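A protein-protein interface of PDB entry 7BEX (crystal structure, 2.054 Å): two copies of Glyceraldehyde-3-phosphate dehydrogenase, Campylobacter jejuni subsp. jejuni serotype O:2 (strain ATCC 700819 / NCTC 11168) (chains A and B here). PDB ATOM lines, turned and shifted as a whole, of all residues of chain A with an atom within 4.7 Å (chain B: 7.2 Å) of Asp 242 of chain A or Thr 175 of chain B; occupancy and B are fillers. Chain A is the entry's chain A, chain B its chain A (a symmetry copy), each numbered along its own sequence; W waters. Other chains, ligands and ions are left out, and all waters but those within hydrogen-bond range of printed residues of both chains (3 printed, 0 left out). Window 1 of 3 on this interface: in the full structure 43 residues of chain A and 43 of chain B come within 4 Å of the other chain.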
ATOM      1  N   LEU A 173       3.501  17.758 -29.918  1.00  0.00           N
ATOM      2  CA  LEU A 173       4.343  18.567 -29.022  1.00  0.00           C
ATOM      3  C   LEU A 173       3.992  18.158 -27.593  1.00  0.00           C
ATOM      4  O   LEU A 173       2.804  17.851 -27.314  1.00  0.00           O
ATOM      5  CB  LEU A 173       4.100  20.046 -29.323  1.00  0.00           C
ATOM      6  CG  LEU A 173       4.615  20.559 -30.674  1.00  0.00           C
ATOM      7  CD1 LEU A 173       4.157  21.992 -30.908  1.00  0.00           C
ATOM      8  CD2 LEU A 173       6.121  20.482 -30.685  1.00  0.00           C
ATOM      9  N   MET A 174       5.015  18.028 -26.774  1.00  0.00           N
ATOM     10  CA  MET A 174       4.922  17.500 -25.404  1.00  0.00           C
ATOM     11  C   MET A 174       5.326  18.594 -24.427  1.00  0.00           C
ATOM     12  O   MET A 174       6.335  19.309 -24.663  1.00  0.00           O
ATOM     13  CB  MET A 174       5.860  16.305 -25.209  1.00  0.00           C
ATOM     14  CG  MET A 174       6.119  16.028 -23.721  1.00  0.00           C
ATOM     15  SD  MET A 174       7.375  14.828 -23.474  1.00  0.00           S
ATOM     16  CE  MET A 174       8.733  15.975 -23.738  1.00  0.00           C
ATOM     17  N   THR A 175       4.628  18.675 -23.302  1.00  0.00           N
ATOM     18  CA  THR A 175       5.127  19.381 -22.103  1.00  0.00           C
ATOM     19  C   THR A 175       5.158  18.345 -20.989  1.00  0.00           C
ATOM     20  O   THR A 175       4.123  17.658 -20.803  1.00  0.00           O
ATOM     21  CB  THR A 175       4.242  20.577 -21.729  1.00  0.00           C
ATOM     22  OG1 THR A 175       4.165  21.518 -22.801  1.00  0.00           O
ATOM     23  CG2 THR A 175       4.708  21.265 -20.462  1.00  0.00           C
ATOM     24  N   ILE A 177       5.147  18.284 -17.016  1.00  0.00           N
ATOM     25  CA  ILE A 177       4.976  18.965 -15.719  1.00  0.00           C
ATOM     26  C   ILE A 177       5.755  18.118 -14.735  1.00  0.00           C
ATOM     27  O   ILE A 177       5.325  16.965 -14.425  1.00  0.00           O
ATOM     28  CB  ILE A 177       3.496  19.125 -15.327  1.00  0.00           C
ATOM     29  CG1 ILE A 177       2.723  19.913 -16.386  1.00  0.00           C
ATOM     30  CG2 ILE A 177       3.448  19.772 -13.936  1.00  0.00           C
ATOM     31  CD1 ILE A 177       1.193  19.709 -16.326  1.00  0.00           C
ATOM     32  N   SER A 240       4.347  14.465 -15.069  1.00  0.00           N
ATOM     33  CA  SER A 240       3.391  14.011 -16.111  1.00  0.00           C
ATOM     34  C   SER A 240       3.868  14.412 -17.509  1.00  0.00           C
ATOM     35  O   SER A 240       4.340  15.581 -17.721  1.00  0.00           O
ATOM     36  CB  SER A 240       1.983  14.513 -15.851  1.00  0.00           C
ATOM     37  OG  SER A 240       1.940  15.910 -15.745  1.00  0.00           O
ATOM     38  N   VAL A 241       3.719  13.497 -18.441  1.00  0.00           N
ATOM     39  CA  VAL A 241       3.788  13.789 -19.893  1.00  0.00           C
ATOM     40  C   VAL A 241       2.415  14.322 -20.325  1.00  0.00           C
ATOM     41  O   VAL A 241       1.396  13.621 -20.062  1.00  0.00           O
ATOM     42  CB  VAL A 241       4.208  12.555 -20.690  1.00  0.00           C
ATOM     43  CG1 VAL A 241       3.906  12.722 -22.182  1.00  0.00           C
ATOM     44  CG2 VAL A 241       5.678  12.188 -20.444  1.00  0.00           C
ATOM     45  N   ASP A 242       2.398  15.519 -20.926  1.00  0.00           N
ATOM     46  CA  ASP A 242       1.201  16.116 -21.538  1.00  0.00           C
ATOM     47  C   ASP A 242       1.504  16.146 -23.044  1.00  0.00           C
ATOM     48  O   ASP A 242       2.277  17.016 -23.457  1.00  0.00           O
ATOM     49  CB  ASP A 242       0.868  17.444 -20.859  1.00  0.00           C
ATOM     50  CG  ASP A 242      -0.297  18.193 -21.477  1.00  0.00           C
ATOM     51  OD1 ASP A 242      -0.783  17.757 -22.537  1.00  0.00           O
ATOM     52  OD2 ASP A 242      -0.643  19.246 -20.956  1.00  0.00           O
ATOM     53  N   LEU A 243       1.013  15.141 -23.781  1.00  0.00           N
ATOM     54  CA  LEU A 243       1.303  14.955 -25.221  1.00  0.00           C
ATOM     55  C   LEU A 243       0.102  15.438 -26.005  1.00  0.00           C
ATOM     56  O   LEU A 243      -0.987  14.896 -25.806  1.00  0.00           O
ATOM     57  CB  LEU A 243       1.591  13.497 -25.578  1.00  0.00           C
ATOM     58  CG  LEU A 243       1.751  13.233 -27.073  1.00  0.00           C
ATOM     59  CD1 LEU A 243       2.925  14.007 -27.633  1.00  0.00           C
ATOM     60  CD2 LEU A 243       1.956  11.745 -27.331  1.00  0.00           C
ATOM     61  N   THR A 244       0.318  16.374 -26.913  1.00  0.00           N
ATOM     62  CA  THR A 244      -0.736  16.835 -27.836  1.00  0.00           C
ATOM     63  C   THR A 244      -0.297  16.439 -29.221  1.00  0.00           C
ATOM     64  O   THR A 244       0.819  16.739 -29.550  1.00  0.00           O
ATOM     65  CB  THR A 244      -1.019  18.336 -27.756  1.00  0.00           C
ATOM     66  OG1 THR A 244      -1.179  18.723 -26.401  1.00  0.00           O
ATOM     67  CG2 THR A 244      -2.266  18.681 -28.538  1.00  0.00           C
ATOM     68  N   LYS A 307      -5.049  14.927 -26.834  1.00  0.00           N
ATOM     69  CA  LYS A 307      -4.181  15.137 -25.658  1.00  0.00           C
ATOM     70  C   LYS A 307      -4.258  13.922 -24.746  1.00  0.00           C
ATOM     71  O   LYS A 307      -5.382  13.482 -24.446  1.00  0.00           O
ATOM     72  CB  LYS A 307      -4.612  16.366 -24.875  1.00  0.00           C
ATOM     73  CG  LYS A 307      -3.771  16.680 -23.643  1.00  0.00           C
ATOM     74  CD  LYS A 307      -4.188  17.927 -22.903  1.00  0.00           C
ATOM     75  CE  LYS A 307      -4.017  19.189 -23.703  1.00  0.00           C
ATOM     76  NZ  LYS A 307      -2.604  19.593 -23.787  1.00  0.00           N
ATOM     77  N   VAL A 308      -3.091  13.443 -24.330  1.00  0.00           N
ATOM     78  CA  VAL A 308      -2.889  12.337 -23.367  1.00  0.00           C
ATOM     79  C   VAL A 308      -2.008  12.884 -22.247  1.00  0.00           C
ATOM     80  O   VAL A 308      -0.969  13.522 -22.533  1.00  0.00           O
ATOM     81  CB  VAL A 308      -2.309  11.121 -24.077  1.00  0.00           C
ATOM     82  CG1 VAL A 308      -1.786  10.084 -23.095  1.00  0.00           C
ATOM     83  CG2 VAL A 308      -3.369  10.522 -24.996  1.00  0.00           C
ATOM     84  N   ILE A 309      -2.491  12.739 -21.026  1.00  0.00           N
ATOM     85  CA  ILE A 309      -1.736  12.993 -19.779  1.00  0.00           C
ATOM     86  C   ILE A 309      -1.394  11.659 -19.113  1.00  0.00           C
ATOM     87  O   ILE A 309      -2.326  10.877 -18.721  1.00  0.00           O
ATOM     88  CB  ILE A 309      -2.524  13.979 -18.895  1.00  0.00           C
ATOM     89  CG1 ILE A 309      -2.700  15.287 -19.690  1.00  0.00           C
ATOM     90  CG2 ILE A 309      -1.799  14.170 -17.585  1.00  0.00           C
ATOM     91  CD1 ILE A 309      -3.227  16.429 -18.938  1.00  0.00           C
ATOM     92  N   THR B 152      -8.185  32.584 -16.774  1.00  0.00           N
ATOM     93  CA  THR B 152      -7.650  31.798 -17.920  1.00  0.00           C
ATOM     94  C   THR B 152      -8.100  32.399 -19.255  1.00  0.00           C
ATOM     95  O   THR B 152      -7.272  32.481 -20.186  1.00  0.00           O
ATOM     96  CB  THR B 152      -8.003  30.316 -17.758  1.00  0.00           C
ATOM     97  OG1 THR B 152      -7.405  29.919 -16.513  1.00  0.00           O
ATOM     98  CG2 THR B 152      -7.462  29.478 -18.903  1.00  0.00           C
ATOM     99  N   LEU B 173      -5.713  22.461 -28.222  1.00  0.00           N
ATOM    100  CA  LEU B 173      -5.988  21.951 -26.869  1.00  0.00           C
ATOM    101  C   LEU B 173      -5.037  22.677 -25.920  1.00  0.00           C
ATOM    102  O   LEU B 173      -3.877  22.969 -26.312  1.00  0.00           O
ATOM    103  CB  LEU B 173      -5.822  20.432 -26.873  1.00  0.00           C
ATOM    104  CG  LEU B 173      -6.874  19.635 -27.655  1.00  0.00           C
ATOM    105  CD1 LEU B 173      -6.490  18.162 -27.715  1.00  0.00           C
ATOM    106  CD2 LEU B 173      -8.213  19.800 -26.982  1.00  0.00           C
ATOM    107  N   MET B 174      -5.566  23.068 -24.779  1.00  0.00           N
ATOM    108  CA  MET B 174      -4.878  23.910 -23.787  1.00  0.00           C
ATOM    109  C   MET B 174      -4.711  23.118 -22.500  1.00  0.00           C
ATOM    110  O   MET B 174      -5.667  22.431 -22.054  1.00  0.00           O
ATOM    111  CB  MET B 174      -5.689  25.172 -23.479  1.00  0.00           C
ATOM    112  CG  MET B 174      -5.241  25.822 -22.162  1.00  0.00           C
ATOM    113  SD  MET B 174      -6.309  27.122 -21.662  1.00  0.00           S
ATOM    114  CE  MET B 174      -7.559  26.032 -20.971  1.00  0.00           C
ATOM    115  N   THR B 175      -3.566  23.273 -21.849  1.00  0.00           N
ATOM    116  CA  THR B 175      -3.403  22.916 -20.424  1.00  0.00           C
ATOM    117  C   THR B 175      -2.976  24.194 -19.718  1.00  0.00           C
ATOM    118  O   THR B 175      -2.018  24.841 -20.212  1.00  0.00           O
ATOM    119  CB  THR B 175      -2.374  21.797 -20.224  1.00  0.00           C
ATOM    120  OG1 THR B 175      -2.747  20.618 -20.939  1.00  0.00           O
ATOM    121  CG2 THR B 175      -2.152  21.472 -18.760  1.00  0.00           C
ATOM    122  N   THR B 176      -3.632  24.545 -18.610  1.00  0.00           N
ATOM    123  CA  THR B 176      -3.111  25.553 -17.681  1.00  0.00           C
ATOM    124  C   THR B 176      -2.358  24.838 -16.570  1.00  0.00           C
ATOM    125  O   THR B 176      -2.950  23.983 -15.888  1.00  0.00           O
ATOM    126  CB  THR B 176      -4.208  26.491 -17.184  1.00  0.00           C
ATOM    127  OG1 THR B 176      -5.253  25.722 -16.584  1.00  0.00           O
ATOM    128  CG2 THR B 176      -4.801  27.285 -18.322  1.00  0.00           C
ATOM    129  N   ILE B 177      -1.118  25.231 -16.362  1.00  0.00           N
ATOM    130  CA  ILE B 177      -0.320  24.881 -15.171  1.00  0.00           C
ATOM    131  C   ILE B 177      -0.601  25.992 -14.181  1.00  0.00           C
ATOM    132  O   ILE B 177      -0.148  27.156 -14.403  1.00  0.00           O
ATOM    133  CB  ILE B 177       1.179  24.731 -15.490  1.00  0.00           C
ATOM    134  CG1 ILE B 177       1.416  23.660 -16.556  1.00  0.00           C
ATOM    135  CG2 ILE B 177       1.910  24.445 -14.171  1.00  0.00           C
ATOM    136  CD1 ILE B 177       2.782  23.777 -17.268  1.00  0.00           C
ATOM    137  N   HIS B 178      -1.485  25.688 -13.242  1.00  0.00           N
ATOM    138  CA  HIS B 178      -2.203  26.689 -12.460  1.00  0.00           C
ATOM    139  C   HIS B 178      -1.833  26.646 -10.980  1.00  0.00           C
ATOM    140  O   HIS B 178      -1.762  25.563 -10.411  1.00  0.00           O
ATOM    141  CB  HIS B 178      -3.676  26.446 -12.708  1.00  0.00           C
ATOM    142  CG  HIS B 178      -4.552  27.593 -12.377  1.00  0.00           C
ATOM    143  ND1 HIS B 178      -4.740  28.014 -11.066  1.00  0.00           N
ATOM    144  CD2 HIS B 178      -5.378  28.329 -13.164  1.00  0.00           C
ATOM    145  CE1 HIS B 178      -5.640  28.976 -11.064  1.00  0.00           C
ATOM    146  NE2 HIS B 178      -6.068  29.190 -12.346  1.00  0.00           N
ATOM    147  N   THR B 209     -11.330  23.036 -16.583  1.00  0.00           N
ATOM    148  CA  THR B 209     -11.585  24.461 -16.901  1.00  0.00           C
ATOM    149  C   THR B 209     -12.448  24.436 -18.162  1.00  0.00           C
ATOM    150  O   THR B 209     -12.095  23.670 -19.078  1.00  0.00           O
ATOM    151  CB  THR B 209     -10.284  25.248 -17.156  1.00  0.00           C
ATOM    152  OG1 THR B 209     -10.637  26.449 -17.834  1.00  0.00           O
ATOM    153  CG2 THR B 209      -9.276  24.572 -18.064  1.00  0.00           C
ATOM    154  N   HIS B 227     -10.532  22.817 -26.722  1.00  0.00           N
ATOM    155  CA  HIS B 227     -10.849  22.251 -25.385  1.00  0.00           C
ATOM    156  C   HIS B 227      -9.610  22.491 -24.511  1.00  0.00           C
ATOM    157  O   HIS B 227      -8.504  22.845 -25.074  1.00  0.00           O
ATOM    158  CB  HIS B 227     -11.175  20.736 -25.408  1.00  0.00           C
ATOM    159  CG  HIS B 227     -12.465  20.293 -26.026  1.00  0.00           C
ATOM    160  ND1 HIS B 227     -12.545  19.152 -26.852  1.00  0.00           N
ATOM    161  CD2 HIS B 227     -13.730  20.762 -25.930  1.00  0.00           C
ATOM    162  CE1 HIS B 227     -13.790  18.983 -27.255  1.00  0.00           C
ATOM    163  NE2 HIS B 227     -14.527  19.968 -26.720  1.00  0.00           N
ATOM    164  N   GLY B 228      -9.736  22.244 -23.230  1.00  0.00           N
ATOM    165  CA  GLY B 228      -8.602  22.445 -22.324  1.00  0.00           C
ATOM    166  C   GLY B 228      -8.833  21.795 -20.988  1.00  0.00           C
ATOM    167  O   GLY B 228      -9.912  21.216 -20.746  1.00  0.00           O
ATOM    168  N   GLN B 229      -7.795  21.857 -20.173  1.00  0.00           N
ATOM    169  CA  GLN B 229      -7.827  21.298 -18.824  1.00  0.00           C
ATOM    170  C   GLN B 229      -6.769  22.010 -18.010  1.00  0.00           C
ATOM    171  O   GLN B 229      -5.969  22.752 -18.568  1.00  0.00           O
ATOM    172  CB  GLN B 229      -7.695  19.773 -18.858  1.00  0.00           C
ATOM    173  CG  GLN B 229      -6.491  19.248 -19.580  1.00  0.00           C
ATOM    174  CD  GLN B 229      -6.503  17.726 -19.499  1.00  0.00           C
ATOM    175  OE1 GLN B 229      -6.236  17.160 -18.430  1.00  0.00           O
ATOM    176  NE2 GLN B 229      -6.799  17.054 -20.619  1.00  0.00           N
ATOM    177  N   SER B 230      -6.827  21.806 -16.720  1.00  0.00           N
ATOM    178  CA  SER B 230      -5.926  22.453 -15.752  1.00  0.00           C
ATOM    179  C   SER B 230      -5.159  21.394 -14.967  1.00  0.00           C
ATOM    180  O   SER B 230      -5.674  20.283 -14.755  1.00  0.00           O
ATOM    181  CB  SER B 230      -6.735  23.371 -14.888  1.00  0.00           C
ATOM    182  OG  SER B 230      -5.866  24.137 -14.086  1.00  0.00           O
ATOM    183  N   MET B 231      -3.920  21.720 -14.625  1.00  0.00           N
ATOM    184  CA  MET B 231      -3.055  20.945 -13.726  1.00  0.00           C
ATOM    185  C   MET B 231      -2.624  21.896 -12.609  1.00  0.00           C
ATOM    186  O   MET B 231      -1.853  22.797 -12.886  1.00  0.00           O
ATOM    187  CB  MET B 231      -1.861  20.396 -14.507  1.00  0.00           C
ATOM    188  CG  MET B 231      -2.281  19.440 -15.607  1.00  0.00           C
ATOM    189  SD  MET B 231      -2.882  17.837 -14.951  1.00  0.00           S
ATOM    190  CE  MET B 231      -1.315  16.962 -14.840  1.00  0.00           C
ATOM    191  N   SER B 240       0.259  29.355 -16.021  1.00  0.00           N
ATOM    192  CA  SER B 240       0.589  29.478 -17.464  1.00  0.00           C
ATOM    193  C   SER B 240      -0.459  28.776 -18.330  1.00  0.00           C
ATOM    194  O   SER B 240      -0.902  27.622 -18.003  1.00  0.00           O
ATOM    195  CB  SER B 240       1.984  28.970 -17.776  1.00  0.00           C
ATOM    196  OG  SER B 240       2.158  27.641 -17.362  1.00  0.00           O
ATOM    197  N   VAL B 241      -0.819  29.422 -19.417  1.00  0.00           N
ATOM    198  CA  VAL B 241      -1.538  28.787 -20.547  1.00  0.00           C
ATOM    199  C   VAL B 241      -0.495  28.079 -21.423  1.00  0.00           C
ATOM    200  O   VAL B 241       0.483  28.758 -21.847  1.00  0.00           O
ATOM    201  CB  VAL B 241      -2.357  29.810 -21.333  1.00  0.00           C
ATOM    202  CG1 VAL B 241      -2.776  29.262 -22.700  1.00  0.00           C
ATOM    203  CG2 VAL B 241      -3.562  30.317 -20.529  1.00  0.00           C
ATOM    204  N   ASP B 242      -0.685  26.772 -21.647  1.00  0.00           N
ATOM    205  CA  ASP B 242       0.122  25.970 -22.579  1.00  0.00           C
ATOM    206  C   ASP B 242      -0.845  25.588 -23.709  1.00  0.00           C
ATOM    207  O   ASP B 242      -1.666  24.693 -23.485  1.00  0.00           O
ATOM    208  CB  ASP B 242       0.815  24.831 -21.829  1.00  0.00           C
ATOM    209  CG  ASP B 242       1.602  23.883 -22.713  1.00  0.00           C
ATOM    210  OD1 ASP B 242       1.509  24.013 -23.948  1.00  0.00           O
ATOM    211  OD2 ASP B 242       2.215  22.971 -22.172  1.00  0.00           O
ATOM    212  N   LEU B 243      -0.818  26.349 -24.812  1.00  0.00           N
ATOM    213  CA  LEU B 243      -1.756  26.192 -25.946  1.00  0.00           C
ATOM    214  C   LEU B 243      -1.032  25.457 -27.053  1.00  0.00           C
ATOM    215  O   LEU B 243      -0.012  25.963 -27.525  1.00  0.00           O
ATOM    216  CB  LEU B 243      -2.268  27.533 -26.474  1.00  0.00           C
ATOM    217  CG  LEU B 243      -3.123  27.430 -27.735  1.00  0.00           C
ATOM    218  CD1 LEU B 243      -4.372  26.615 -27.472  1.00  0.00           C
ATOM    219  CD2 LEU B 243      -3.516  28.818 -28.225  1.00  0.00           C
ATOM    220  N   THR B 244      -1.588  24.341 -27.494  1.00  0.00           N
ATOM    221  CA  THR B 244      -1.060  23.603 -28.656  1.00  0.00           C
ATOM    222  C   THR B 244      -2.117  23.672 -29.725  1.00  0.00           C
ATOM    223  O   THR B 244      -3.237  23.370 -29.410  1.00  0.00           O
ATOM    224  CB  THR B 244      -0.680  22.154 -28.350  1.00  0.00           C
ATOM    225  OG1 THR B 244       0.118  22.104 -27.178  1.00  0.00           O
ATOM    226  CG2 THR B 244       0.078  21.550 -29.511  1.00  0.00           C
ATOM    227  N   LYS B 307       3.095  25.427 -30.285  1.00  0.00           N
ATOM    228  CA  LYS B 307       2.891  25.568 -28.829  1.00  0.00           C
ATOM    229  C   LYS B 307       3.308  26.963 -28.389  1.00  0.00           C
ATOM    230  O   LYS B 307       4.412  27.393 -28.767  1.00  0.00           O
ATOM    231  CB  LYS B 307       3.712  24.545 -28.061  1.00  0.00           C
ATOM    232  CG  LYS B 307       3.564  24.598 -26.546  1.00  0.00           C
ATOM    233  CD  LYS B 307       4.354  23.548 -25.804  1.00  0.00           C
ATOM    234  CE  LYS B 307       3.909  22.141 -26.094  1.00  0.00           C
ATOM    235  NZ  LYS B 307       2.647  21.817 -25.406  1.00  0.00           N
ATOM    236  N   VAL B 308       2.443  27.602 -27.610  1.00  0.00           N
ATOM    237  CA  VAL B 308       2.644  28.921 -26.969  1.00  0.00           C
ATOM    238  C   VAL B 308       2.424  28.722 -25.473  1.00  0.00           C
ATOM    239  O   VAL B 308       1.413  28.099 -25.074  1.00  0.00           O
ATOM    240  CB  VAL B 308       1.726  29.958 -27.601  1.00  0.00           C
ATOM    241  CG1 VAL B 308       1.658  31.235 -26.779  1.00  0.00           C
ATOM    242  CG2 VAL B 308       2.196  30.245 -29.025  1.00  0.00           C
ATOM    243  N   TYR B 312       0.339  34.176 -16.549  1.00  0.00           N
ATOM    244  CA  TYR B 312      -0.654  35.140 -16.030  1.00  0.00           C
ATOM    245  C   TYR B 312      -0.628  35.072 -14.507  1.00  0.00           C
ATOM    246  O   TYR B 312      -0.656  33.944 -13.976  1.00  0.00           O
ATOM    247  CB  TYR B 312      -2.038  34.898 -16.639  1.00  0.00           C
ATOM    248  CG  TYR B 312      -2.719  33.561 -16.449  1.00  0.00           C
ATOM    249  CD1 TYR B 312      -2.210  32.386 -17.002  1.00  0.00           C
ATOM    250  CD2 TYR B 312      -3.967  33.500 -15.856  1.00  0.00           C
ATOM    251  CE1 TYR B 312      -2.870  31.172 -16.887  1.00  0.00           C
ATOM    252  CE2 TYR B 312      -4.628  32.287 -15.712  1.00  0.00           C
ATOM    253  CZ  TYR B 312      -4.072  31.114 -16.208  1.00  0.00           C
ATOM    254  OH  TYR B 312      -4.764  29.938 -16.123  1.00  0.00           O
HETATM  255  O   HOH W   1      -1.325  22.080 -24.755  1.00  0.00           O
HETATM  256  O   HOH W   2       0.498  20.957 -22.707  1.00  0.00           O
HETATM  257  O   HOH W   3       1.222  19.253 -25.021  1.00  0.00           O
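OD2 of Asp 242 of chain B sits at hydrogen-bond distance from OG1 of Thr 175 of chain A, 2.5 Å away. OG1 of Thr 175 of chain A is in hydrogen-bond range of NZ of Lys 307 of chain B (3.0 Å). The side-chain carboxylate (OD2) of Asp 242 of chain A lies within hydrogen-bond range of the side-chain hydroxyl (OG1) of Thr 175 of chain B. The side-chain hydroxyl of Thr 175 of chain B sits at hydrogen-bond distance from the side-chain amino group of Lys 307 of chain A (3.0 Å).
The side-chain carboxylate (OD1) of Asp 242 of chain A is in salt-bridge range of the side-chain amino group (NZ) of Lys 307 of chain A. O of His 227 of chain B is in hydrogen-bond range of N of Met 174 of chain B (3.0 Å). The backbone carbonyl oxygen of Thr 175 of chain B is in hydrogen-bond range of the backbone NH of Asp 242 of chain B (2.8 Å). O of Thr 176 of chain B is in hydrogen-bond range of N of Met 231 of chain B (2.8 Å). The backbone NH (N) of Ser 240 of chain B is in hydrogen-bond range of the backbone carbonyl oxygen (O) of Ile 177 of chain B, at 2.8 Å. The backbone NH (N) of His 178 of chain B sits at hydrogen-bond distance from the backbone carbonyl oxygen (O) of Met 231 of chain B, 2.9 Å away.
Leu 173 of chain A touches Lys 307 of chain B (CD1 to N, 3.6 Å). Lys 307 of chain B touches Met 174 of chain A. Ile 177 of chain A touches Ile 177 of chain B. CG of Met 231 of chain B touches CD1 of Ile 177 of chain A, 3.6 Å away. Ser 240 of chain A touches Met 231 of chain B (OG to CE, 3.5 Å). OG1 of Thr 244 of chain B touches OG1 of Thr 244 of chain A (3.7 Å). Lys 307 of chain A touches Leu 173 of chain B. Lys 307 of chain A touches Met 174 of chain B (CE to O, 3.99 Å). NE2 of Gln 229 of chain B touches CD of Lys 307 of chain A (3.6 Å). Met 231 of chain B touches Ile 309 of chain A.
Printed residues of chain B within 4 Å of Met 174 of chain A: Lys 307. Printed residues of chain B within 4 Å of Ser 240 of chain A: Met 231 (3.5 Å). Asp 242 of chain A touches just one residue of chain B: Thr 175 (2.5 Å). Printed residues of chain B within 4 Å of Lys 307 of chain A: Leu 173 (3.6 Å), Met 174 (3.99 Å), Thr 175 (3.0 Å) and Gln 229 (3.6 Å). Printed residues of chain B within 4 Å of Ile 309 of chain A: Gln 229 and Met 231. Thr 175 of chain B touches just these residues of chain A: Asp 242 and Lys 307. Of the printed residues of chain A, Gln 229 of chain B touches Lys 307 (3.6 Å) and Ile 309 (3.1 Å). The nearest residue of chain B that does not touch Asp 242 of chain A is Asp 242 of chain B (4.8 Å).
Printed residues of chain A that touch a printed residue of chain B: Leu 173, Met 174, Thr 175, Ile 177, Ser 240, Asp 242, Thr 244, Lys 307 and Ile 309. Among the printed residues, 15 pairs touch across the chains. Among the printed residues, no Asp or Glu carboxylate lies within 4 Å of a Lys or Arg side-chain nitrogen of the other chain.
Met 174 of chain A touches Lys 307 of chain B, and with the chains exchanged Lys 307 of chain A touches Met 174 of chain B. Thr 175 of chain A touches Lys 307 of chain B, and with the chains exchanged Lys 307 of chain A touches Thr 175 of chain B. Ile 177 of chain A touches its own counterpart, Ile 177 of chain B. Thr 244 of chain A touches its own counterpart, Thr 244 of chain B. Positions printed for both chains: 173, 174, 175, 177, 240, 241, 242, 243, 244, 307 and 308.
Water W2 lies within hydrogen-bond range of the side-chain carboxylate of Asp 242 of chain A (2.7 Å) and the side-chain carboxylate of Asp 242 of chain B (2.7 Å). Water W3 lies within hydrogen-bond range of the side-chain hydroxyl of Thr 244 of chain A, the backbone carbonyl oxygen of Asp 242 of chain A, the side-chain amino group of Lys 307 of chain B and the backbone carbonyl oxygen of Leu 173 of chain A. Water W1 lies within hydrogen-bond range of the side-chain hydroxyl (OG1) of Thr 244 of chain B (2.8 Å), the backbone carbonyl oxygen (O) of Asp 242 of chain B (2.9 Å), the side-chain amino group (NZ) of Lys 307 of chain A (3.0 Å) and the backbone carbonyl oxygen (O) of Leu 173 of chain B (3.1 Å).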
